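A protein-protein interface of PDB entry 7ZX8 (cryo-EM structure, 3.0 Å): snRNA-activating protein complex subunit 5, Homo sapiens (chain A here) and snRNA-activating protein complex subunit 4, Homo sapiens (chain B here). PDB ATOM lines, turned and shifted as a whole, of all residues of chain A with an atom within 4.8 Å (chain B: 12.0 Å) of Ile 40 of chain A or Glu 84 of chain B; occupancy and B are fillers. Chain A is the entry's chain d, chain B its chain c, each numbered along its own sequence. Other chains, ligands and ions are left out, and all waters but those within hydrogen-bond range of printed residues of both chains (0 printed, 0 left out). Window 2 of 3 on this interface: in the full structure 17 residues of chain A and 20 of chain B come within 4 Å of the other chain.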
ATOM      1  N   LEU A  36     -29.778  -7.309  31.091  1.00  0.00           N
ATOM      2  CA  LEU A  36     -28.599  -8.062  30.678  1.00  0.00           C
ATOM      3  C   LEU A  36     -27.979  -7.464  29.426  1.00  0.00           C
ATOM      4  O   LEU A  36     -26.755  -7.346  29.332  1.00  0.00           O
ATOM      5  CB  LEU A  36     -28.958  -9.529  30.429  1.00  0.00           C
ATOM      6  CG  LEU A  36     -29.467 -10.378  31.596  1.00  0.00           C
ATOM      7  CD1 LEU A  36     -29.394 -11.857  31.246  1.00  0.00           C
ATOM      8  CD2 LEU A  36     -28.684 -10.091  32.862  1.00  0.00           C
ATOM      9  N   GLN A  37     -28.805  -7.094  28.446  1.00  0.00           N
ATOM     10  CA  GLN A  37     -28.270  -6.508  27.222  1.00  0.00           C
ATOM     11  C   GLN A  37     -27.510  -5.224  27.527  1.00  0.00           C
ATOM     12  O   GLN A  37     -26.391  -5.015  27.039  1.00  0.00           O
ATOM     13  CB  GLN A  37     -29.396  -6.238  26.219  1.00  0.00           C
ATOM     14  CG  GLN A  37     -30.266  -7.443  25.860  1.00  0.00           C
ATOM     15  CD  GLN A  37     -29.538  -8.770  25.975  1.00  0.00           C
ATOM     16  OE1 GLN A  37     -28.429  -8.931  25.465  1.00  0.00           O
ATOM     17  NE2 GLN A  37     -30.164  -9.731  26.645  1.00  0.00           N
ATOM     18  N   SER A  38     -28.099  -4.354  28.349  1.00  0.00           N
ATOM     19  CA  SER A  38     -27.435  -3.097  28.684  1.00  0.00           C
ATOM     20  C   SER A  38     -26.126  -3.346  29.429  1.00  0.00           C
ATOM     21  O   SER A  38     -25.093  -2.737  29.120  1.00  0.00           O
ATOM     22  CB  SER A  38     -28.374  -2.217  29.508  1.00  0.00           C
ATOM     23  OG  SER A  38     -28.433  -2.656  30.851  1.00  0.00           O
ATOM     24  N   MET A  39     -26.147  -4.249  30.414  1.00  0.00           N
ATOM     25  CA  MET A  39     -24.937  -4.516  31.188  1.00  0.00           C
ATOM     26  C   MET A  39     -23.846  -5.139  30.326  1.00  0.00           C
ATOM     27  O   MET A  39     -22.668  -4.802  30.481  1.00  0.00           O
ATOM     28  CB  MET A  39     -25.245  -5.417  32.387  1.00  0.00           C
ATOM     29  CG  MET A  39     -26.273  -4.872  33.378  1.00  0.00           C
ATOM     30  SD  MET A  39     -26.224  -3.079  33.593  1.00  0.00           S
ATOM     31  CE  MET A  39     -27.969  -2.672  33.615  1.00  0.00           C
ATOM     32  N   ILE A  40     -24.203  -6.054  29.422  1.00  0.00           N
ATOM     33  CA  ILE A  40     -23.181  -6.667  28.580  1.00  0.00           C
ATOM     34  C   ILE A  40     -22.618  -5.644  27.606  1.00  0.00           C
ATOM     35  O   ILE A  40     -21.416  -5.641  27.325  1.00  0.00           O
ATOM     36  CB  ILE A  40     -23.728  -7.909  27.848  1.00  0.00           C
ATOM     37  CG1 ILE A  40     -24.858  -7.530  26.888  1.00  0.00           C
ATOM     38  CG2 ILE A  40     -24.167  -8.960  28.859  1.00  0.00           C
ATOM     39  CD1 ILE A  40     -25.442  -8.705  26.129  1.00  0.00           C
ATOM     40  N   SER A  41     -23.462  -4.756  27.077  1.00  0.00           N
ATOM     41  CA  SER A  41     -22.937  -3.684  26.238  1.00  0.00           C
ATOM     42  C   SER A  41     -21.928  -2.844  27.013  1.00  0.00           C
ATOM     43  O   SER A  41     -20.809  -2.596  26.542  1.00  0.00           O
ATOM     44  CB  SER A  41     -24.083  -2.814  25.719  1.00  0.00           C
ATOM     45  OG  SER A  41     -24.997  -2.505  26.756  1.00  0.00           O
ATOM     46  N   SER A  42     -22.297  -2.431  28.228  1.00  0.00           N
ATOM     47  CA  SER A  42     -21.400  -1.603  29.029  1.00  0.00           C
ATOM     48  C   SER A  42     -20.096  -2.330  29.335  1.00  0.00           C
ATOM     49  O   SER A  42     -19.013  -1.739  29.255  1.00  0.00           O
ATOM     50  CB  SER A  42     -22.095  -1.183  30.324  1.00  0.00           C
ATOM     51  OG  SER A  42     -22.150  -2.259  31.245  1.00  0.00           O
ATOM     52  N   ARG A  43     -20.178  -3.614  29.690  1.00  0.00           N
ATOM     53  CA  ARG A  43     -18.979  -4.357  30.069  1.00  0.00           C
ATOM     54  C   ARG A  43     -18.077  -4.609  28.867  1.00  0.00           C
ATOM     55  O   ARG A  43     -16.860  -4.407  28.947  1.00  0.00           O
ATOM     56  CB  ARG A  43     -19.370  -5.676  30.735  1.00  0.00           C
ATOM     57  CG  ARG A  43     -20.121  -5.517  32.054  1.00  0.00           C
ATOM     58  CD  ARG A  43     -19.190  -5.171  33.209  1.00  0.00           C
ATOM     59  NE  ARG A  43     -18.749  -3.779  33.173  1.00  0.00           N
ATOM     60  CZ  ARG A  43     -19.510  -2.740  33.504  1.00  0.00           C
ATOM     61  NH1 ARG A  43     -20.763  -2.925  33.903  1.00  0.00           N
ATOM     62  NH2 ARG A  43     -19.017  -1.511  33.438  1.00  0.00           N
ATOM     63  N   ARG A  44     -18.649  -5.050  27.744  1.00  0.00           N
ATOM     64  CA  ARG A  44     -17.858  -5.255  26.539  1.00  0.00           C
ATOM     65  C   ARG A  44     -17.287  -3.951  26.004  1.00  0.00           C
ATOM     66  O   ARG A  44     -16.302  -3.983  25.258  1.00  0.00           O
ATOM     67  CB  ARG A  44     -18.703  -5.936  25.458  1.00  0.00           C
ATOM     68  CG  ARG A  44     -19.337  -7.254  25.890  1.00  0.00           C
ATOM     69  CD  ARG A  44     -18.295  -8.340  26.102  1.00  0.00           C
ATOM     70  NE  ARG A  44     -17.918  -8.468  27.507  1.00  0.00           N
ATOM     71  CZ  ARG A  44     -18.668  -9.055  28.436  1.00  0.00           C
ATOM     72  NH1 ARG A  44     -19.846  -9.576  28.116  1.00  0.00           N
ATOM     73  NH2 ARG A  44     -18.240  -9.122  29.688  1.00  0.00           N
ATOM     74  N   GLY A  45     -17.873  -2.809  26.364  1.00  0.00           N
ATOM     75  CA  GLY A  45     -17.266  -1.543  26.004  1.00  0.00           C
ATOM     76  C   GLY A  45     -15.978  -1.234  26.740  1.00  0.00           C
ATOM     77  O   GLY A  45     -15.281  -0.289  26.356  1.00  0.00           O
ATOM     78  N   GLU B  81     -18.961 -16.065  35.205  1.00  0.00           N
ATOM     79  CA  GLU B  81     -17.724 -15.695  34.528  1.00  0.00           C
ATOM     80  C   GLU B  81     -17.994 -14.658  33.441  1.00  0.00           C
ATOM     81  O   GLU B  81     -17.204 -13.737  33.240  1.00  0.00           O
ATOM     82  CB  GLU B  81     -17.044 -16.933  33.931  1.00  0.00           C
ATOM     83  CG  GLU B  81     -17.922 -17.764  33.002  1.00  0.00           C
ATOM     84  CD  GLU B  81     -18.897 -18.652  33.753  1.00  0.00           C
ATOM     85  OE1 GLU B  81     -19.121 -18.406  34.957  1.00  0.00           O
ATOM     86  OE2 GLU B  81     -19.439 -19.595  33.138  1.00  0.00           O
ATOM     87  N   ASP B  82     -19.120 -14.817  32.742  1.00  0.00           N
ATOM     88  CA  ASP B  82     -19.540 -13.898  31.699  1.00  0.00           C
ATOM     89  C   ASP B  82     -21.052 -14.000  31.578  1.00  0.00           C
ATOM     90  O   ASP B  82     -21.595 -15.108  31.686  1.00  0.00           O
ATOM     91  CB  ASP B  82     -18.885 -14.215  30.350  1.00  0.00           C
ATOM     92  CG  ASP B  82     -17.500 -13.607  30.211  1.00  0.00           C
ATOM     93  OD1 ASP B  82     -17.196 -12.631  30.929  1.00  0.00           O
ATOM     94  OD2 ASP B  82     -16.714 -14.107  29.380  1.00  0.00           O
ATOM     95  N   PRO B  83     -21.760 -12.887  31.359  1.00  0.00           N
ATOM     96  CA  PRO B  83     -23.226 -12.965  31.240  1.00  0.00           C
ATOM     97  C   PRO B  83     -23.708 -13.772  30.043  1.00  0.00           C
ATOM     98  O   PRO B  83     -24.889 -14.141  30.015  1.00  0.00           O
ATOM     99  CB  PRO B  83     -23.652 -11.495  31.125  1.00  0.00           C
ATOM    100  CG  PRO B  83     -22.506 -10.714  31.675  1.00  0.00           C
ATOM    101  CD  PRO B  83     -21.287 -11.492  31.307  1.00  0.00           C
ATOM    102  N   GLU B  84     -22.848 -14.050  29.060  1.00  0.00           N
ATOM    103  CA  GLU B  84     -23.282 -14.812  27.892  1.00  0.00           C
ATOM    104  C   GLU B  84     -23.977 -16.105  28.305  1.00  0.00           C
ATOM    105  O   GLU B  84     -24.994 -16.493  27.716  1.00  0.00           O
ATOM    106  CB  GLU B  84     -22.087 -15.114  26.985  1.00  0.00           C
ATOM    107  CG  GLU B  84     -21.219 -13.903  26.664  1.00  0.00           C
ATOM    108  CD  GLU B  84     -22.030 -12.700  26.224  1.00  0.00           C
ATOM    109  OE1 GLU B  84     -22.113 -11.723  26.998  1.00  0.00           O
ATOM    110  OE2 GLU B  84     -22.584 -12.731  25.105  1.00  0.00           O
ATOM    111  N   THR B  85     -23.442 -16.784  29.323  1.00  0.00           N
ATOM    112  CA  THR B  85     -24.135 -17.949  29.864  1.00  0.00           C
ATOM    113  C   THR B  85     -25.497 -17.552  30.416  1.00  0.00           C
ATOM    114  O   THR B  85     -26.480 -18.284  30.253  1.00  0.00           O
ATOM    115  CB  THR B  85     -23.283 -18.620  30.945  1.00  0.00           C
ATOM    116  OG1 THR B  85     -23.851 -19.892  31.282  1.00  0.00           O
ATOM    117  CG2 THR B  85     -23.211 -17.759  32.197  1.00  0.00           C
ATOM    118  N   CYS B  86     -25.578 -16.387  31.065  1.00  0.00           N
ATOM    119  CA  CYS B  86     -26.873 -15.879  31.502  1.00  0.00           C
ATOM    120  C   CYS B  86     -27.797 -15.658  30.315  1.00  0.00           C
ATOM    121  O   CYS B  86     -28.978 -16.022  30.362  1.00  0.00           O
ATOM    122  CB  CYS B  86     -26.693 -14.580  32.289  1.00  0.00           C
ATOM    123  SG  CYS B  86     -28.090 -14.137  33.354  1.00  0.00           S
ATOM    124  N   LEU B  87     -27.274 -15.072  29.236  1.00  0.00           N
ATOM    125  CA  LEU B  87     -28.097 -14.847  28.055  1.00  0.00           C
ATOM    126  C   LEU B  87     -28.680 -16.156  27.538  1.00  0.00           C
ATOM    127  O   LEU B  87     -29.895 -16.271  27.349  1.00  0.00           O
ATOM    128  CB  LEU B  87     -27.277 -14.154  26.964  1.00  0.00           C
ATOM    129  CG  LEU B  87     -26.475 -12.919  27.381  1.00  0.00           C
ATOM    130  CD1 LEU B  87     -25.751 -12.325  26.184  1.00  0.00           C
ATOM    131  CD2 LEU B  87     -27.377 -11.881  28.032  1.00  0.00           C
ATOM    132  N   GLN B  88     -27.830 -17.163  27.318  1.00  0.00           N
ATOM    133  CA  GLN B  88     -28.321 -18.411  26.734  1.00  0.00           C
ATOM    134  C   GLN B  88     -29.261 -19.146  27.686  1.00  0.00           C
ATOM    135  O   GLN B  88     -30.277 -19.712  27.251  1.00  0.00           O
ATOM    136  CB  GLN B  88     -27.146 -19.305  26.328  1.00  0.00           C
ATOM    137  CG  GLN B  88     -26.201 -19.682  27.457  1.00  0.00           C
ATOM    138  CD  GLN B  88     -26.640 -20.926  28.208  1.00  0.00           C
ATOM    139  OE1 GLN B  88     -27.407 -21.740  27.694  1.00  0.00           O
ATOM    140  NE2 GLN B  88     -26.151 -21.079  29.433  1.00  0.00           N
ATOM    141  N   LEU B  89     -28.948 -19.155  28.986  1.00  0.00           N
ATOM    142  CA  LEU B  89     -29.823 -19.831  29.935  1.00  0.00           C
ATOM    143  C   LEU B  89     -31.188 -19.159  29.989  1.00  0.00           C
ATOM    144  O   LEU B  89     -32.223 -19.835  30.055  1.00  0.00           O
ATOM    145  CB  LEU B  89     -29.182 -19.860  31.321  1.00  0.00           C
ATOM    146  CG  LEU B  89     -30.023 -20.531  32.413  1.00  0.00           C
ATOM    147  CD1 LEU B  89     -30.478 -21.919  31.979  1.00  0.00           C
ATOM    148  CD2 LEU B  89     -29.244 -20.613  33.711  1.00  0.00           C
ATOM    149  N   ASN B  90     -31.215 -17.825  29.955  1.00  0.00           N
ATOM    150  CA  ASN B  90     -32.494 -17.130  29.956  1.00  0.00           C
ATOM    151  C   ASN B  90     -33.239 -17.344  28.644  1.00  0.00           C
ATOM    152  O   ASN B  90     -34.469 -17.429  28.645  1.00  0.00           O
ATOM    153  CB  ASN B  90     -32.279 -15.640  30.227  1.00  0.00           C
ATOM    154  CG  ASN B  90     -33.532 -14.954  30.732  1.00  0.00           C
ATOM    155  OD1 ASN B  90     -34.610 -15.549  30.764  1.00  0.00           O
ATOM    156  ND2 ASN B  90     -33.392 -13.703  31.155  1.00  0.00           N
ATOM    157  N   MET B  91     -32.520 -17.460  27.523  1.00  0.00           N
ATOM    158  CA  MET B  91     -33.174 -17.811  26.264  1.00  0.00           C
ATOM    159  C   MET B  91     -33.878 -19.158  26.371  1.00  0.00           C
ATOM    160  O   MET B  91     -35.037 -19.297  25.969  1.00  0.00           O
ATOM    161  CB  MET B  91     -32.162 -17.842  25.114  1.00  0.00           C
ATOM    162  CG  MET B  91     -31.529 -16.507  24.748  1.00  0.00           C
ATOM    163  SD  MET B  91     -32.724 -15.282  24.183  1.00  0.00           S
ATOM    164  CE  MET B  91     -32.873 -14.270  25.647  1.00  0.00           C
ATOM    165  N   VAL B  92     -33.192 -20.169  26.909  1.00  0.00           N
ATOM    166  CA  VAL B  92     -33.806 -21.495  26.981  1.00  0.00           C
ATOM    167  C   VAL B  92     -34.962 -21.497  27.980  1.00  0.00           C
ATOM    168  O   VAL B  92     -35.991 -22.154  27.758  1.00  0.00           O
ATOM    169  CB  VAL B  92     -32.754 -22.570  27.315  1.00  0.00           C
ATOM    170  CG1 VAL B  92     -32.087 -22.294  28.644  1.00  0.00           C
ATOM    171  CG2 VAL B  92     -33.390 -23.955  27.313  1.00  0.00           C
ATOM    172  N   TYR B  93     -34.819 -20.770  29.091  1.00  0.00           N
ATOM    173  CA  TYR B  93     -35.915 -20.677  30.051  1.00  0.00           C
ATOM    174  C   TYR B  93     -37.133 -20.008  29.423  1.00  0.00           C
ATOM    175  O   TYR B  93     -38.271 -20.465  29.604  1.00  0.00           O
ATOM    176  CB  TYR B  93     -35.458 -19.910  31.292  1.00  0.00           C
ATOM    177  CG  TYR B  93     -36.463 -19.907  32.424  1.00  0.00           C
ATOM    178  CD1 TYR B  93     -36.905 -21.096  32.989  1.00  0.00           C
ATOM    179  CD2 TYR B  93     -36.965 -18.715  32.929  1.00  0.00           C
ATOM    180  CE1 TYR B  93     -37.821 -21.098  34.025  1.00  0.00           C
ATOM    181  CE2 TYR B  93     -37.881 -18.708  33.965  1.00  0.00           C
ATOM    182  CZ  TYR B  93     -38.306 -19.901  34.508  1.00  0.00           C
ATOM    183  OH  TYR B  93     -39.217 -19.898  35.539  1.00  0.00           O
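Of chain B, only Cys 86 (3.4 Å) and Leu 87 (3.7 Å) come within 4 Å of Leu 36 of chain A.
No residue of chain B comes within 4 Å of Ser 38 of chain A.
No residue of chain B comes within 4 Å of Met 39 of chain A.
No residue of chain B comes within 4 Å of Ser 42 of chain A.
No residue of chain B comes within 4 Å of Arg 43 of chain A.
Of the printed residues of chain B, Arg 44 of chain A touches Asp 82, Pro 83 and Glu 84.
Printed residues of chain A within 4 Å of Asp 82 of chain B: Arg 44.
Of the printed residues of chain A, Pro 83 of chain B touches Ile 40 and Arg 44.
Thr 85 of chain B touches none of the printed residues of chain A.
Of the printed residues of chain A, Cys 86 of chain B touches Leu 36 (3.4 Å).
Of the printed residues of chain A, Leu 87 of chain B touches Leu 36 (3.7 Å), Gln 37 (3.8 Å) and Ile 40 (3.6 Å).
Of the 13 printed residues of chain B, 5 touch a printed residue of chain A.
Hydrophobic or aromatic side chains of chain B that line the printed part of chain A: Pro 83 and Leu 87.
Of the 10 printed residues of chain A, 4 touch a printed residue of chain B.
Printed residues of chain A that touch a printed residue of chain B: Leu 36, Gln 37, Ile 40 and Arg 44.
Among the printed residues, Asp or Glu carboxylates within 4 Å of a Lys or Arg side-chain nitrogen of the other chain: Arg 44 of chain A with Asp 82 of chain B (3.9 Å) and Arg 44 of chain A with Glu 84 of chain B (3.3 Å).
Among the printed residues, pairs that only touch across the chains: Leu 36 of chain A with Cys 86 of chain B (3.4 Å), Ile 40 of chain A with Pro 83 of chain B (3.4 Å), Ile 40 of chain A with Leu 87 of chain B (3.6 Å), Leu 36 of chain A with Leu 87 of chain B (3.7 Å), Gln 37 of chain A with Leu 87 of chain B (3.8 Å), Ile 40 of chain A with Glu 84 of chain B (3.9 Å) and Arg 44 of chain A with Pro 83 of chain B (3.99 Å).
OD1 of Asp 82 of chain B lies within salt-bridge range of NH2 of Arg 44 of chain A, at 3.9 Å.
The side-chain carboxylate (OE1) of Glu 84 of chain B is in salt-bridge range of the guanidinium group (NH1) of Arg 44 of chain A (3.3 Å).
The side-chain hydroxyl (OG) of Ser 41 of chain A is in hydrogen-bond range of the backbone carbonyl oxygen (O) of Gln 37 of chain A.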
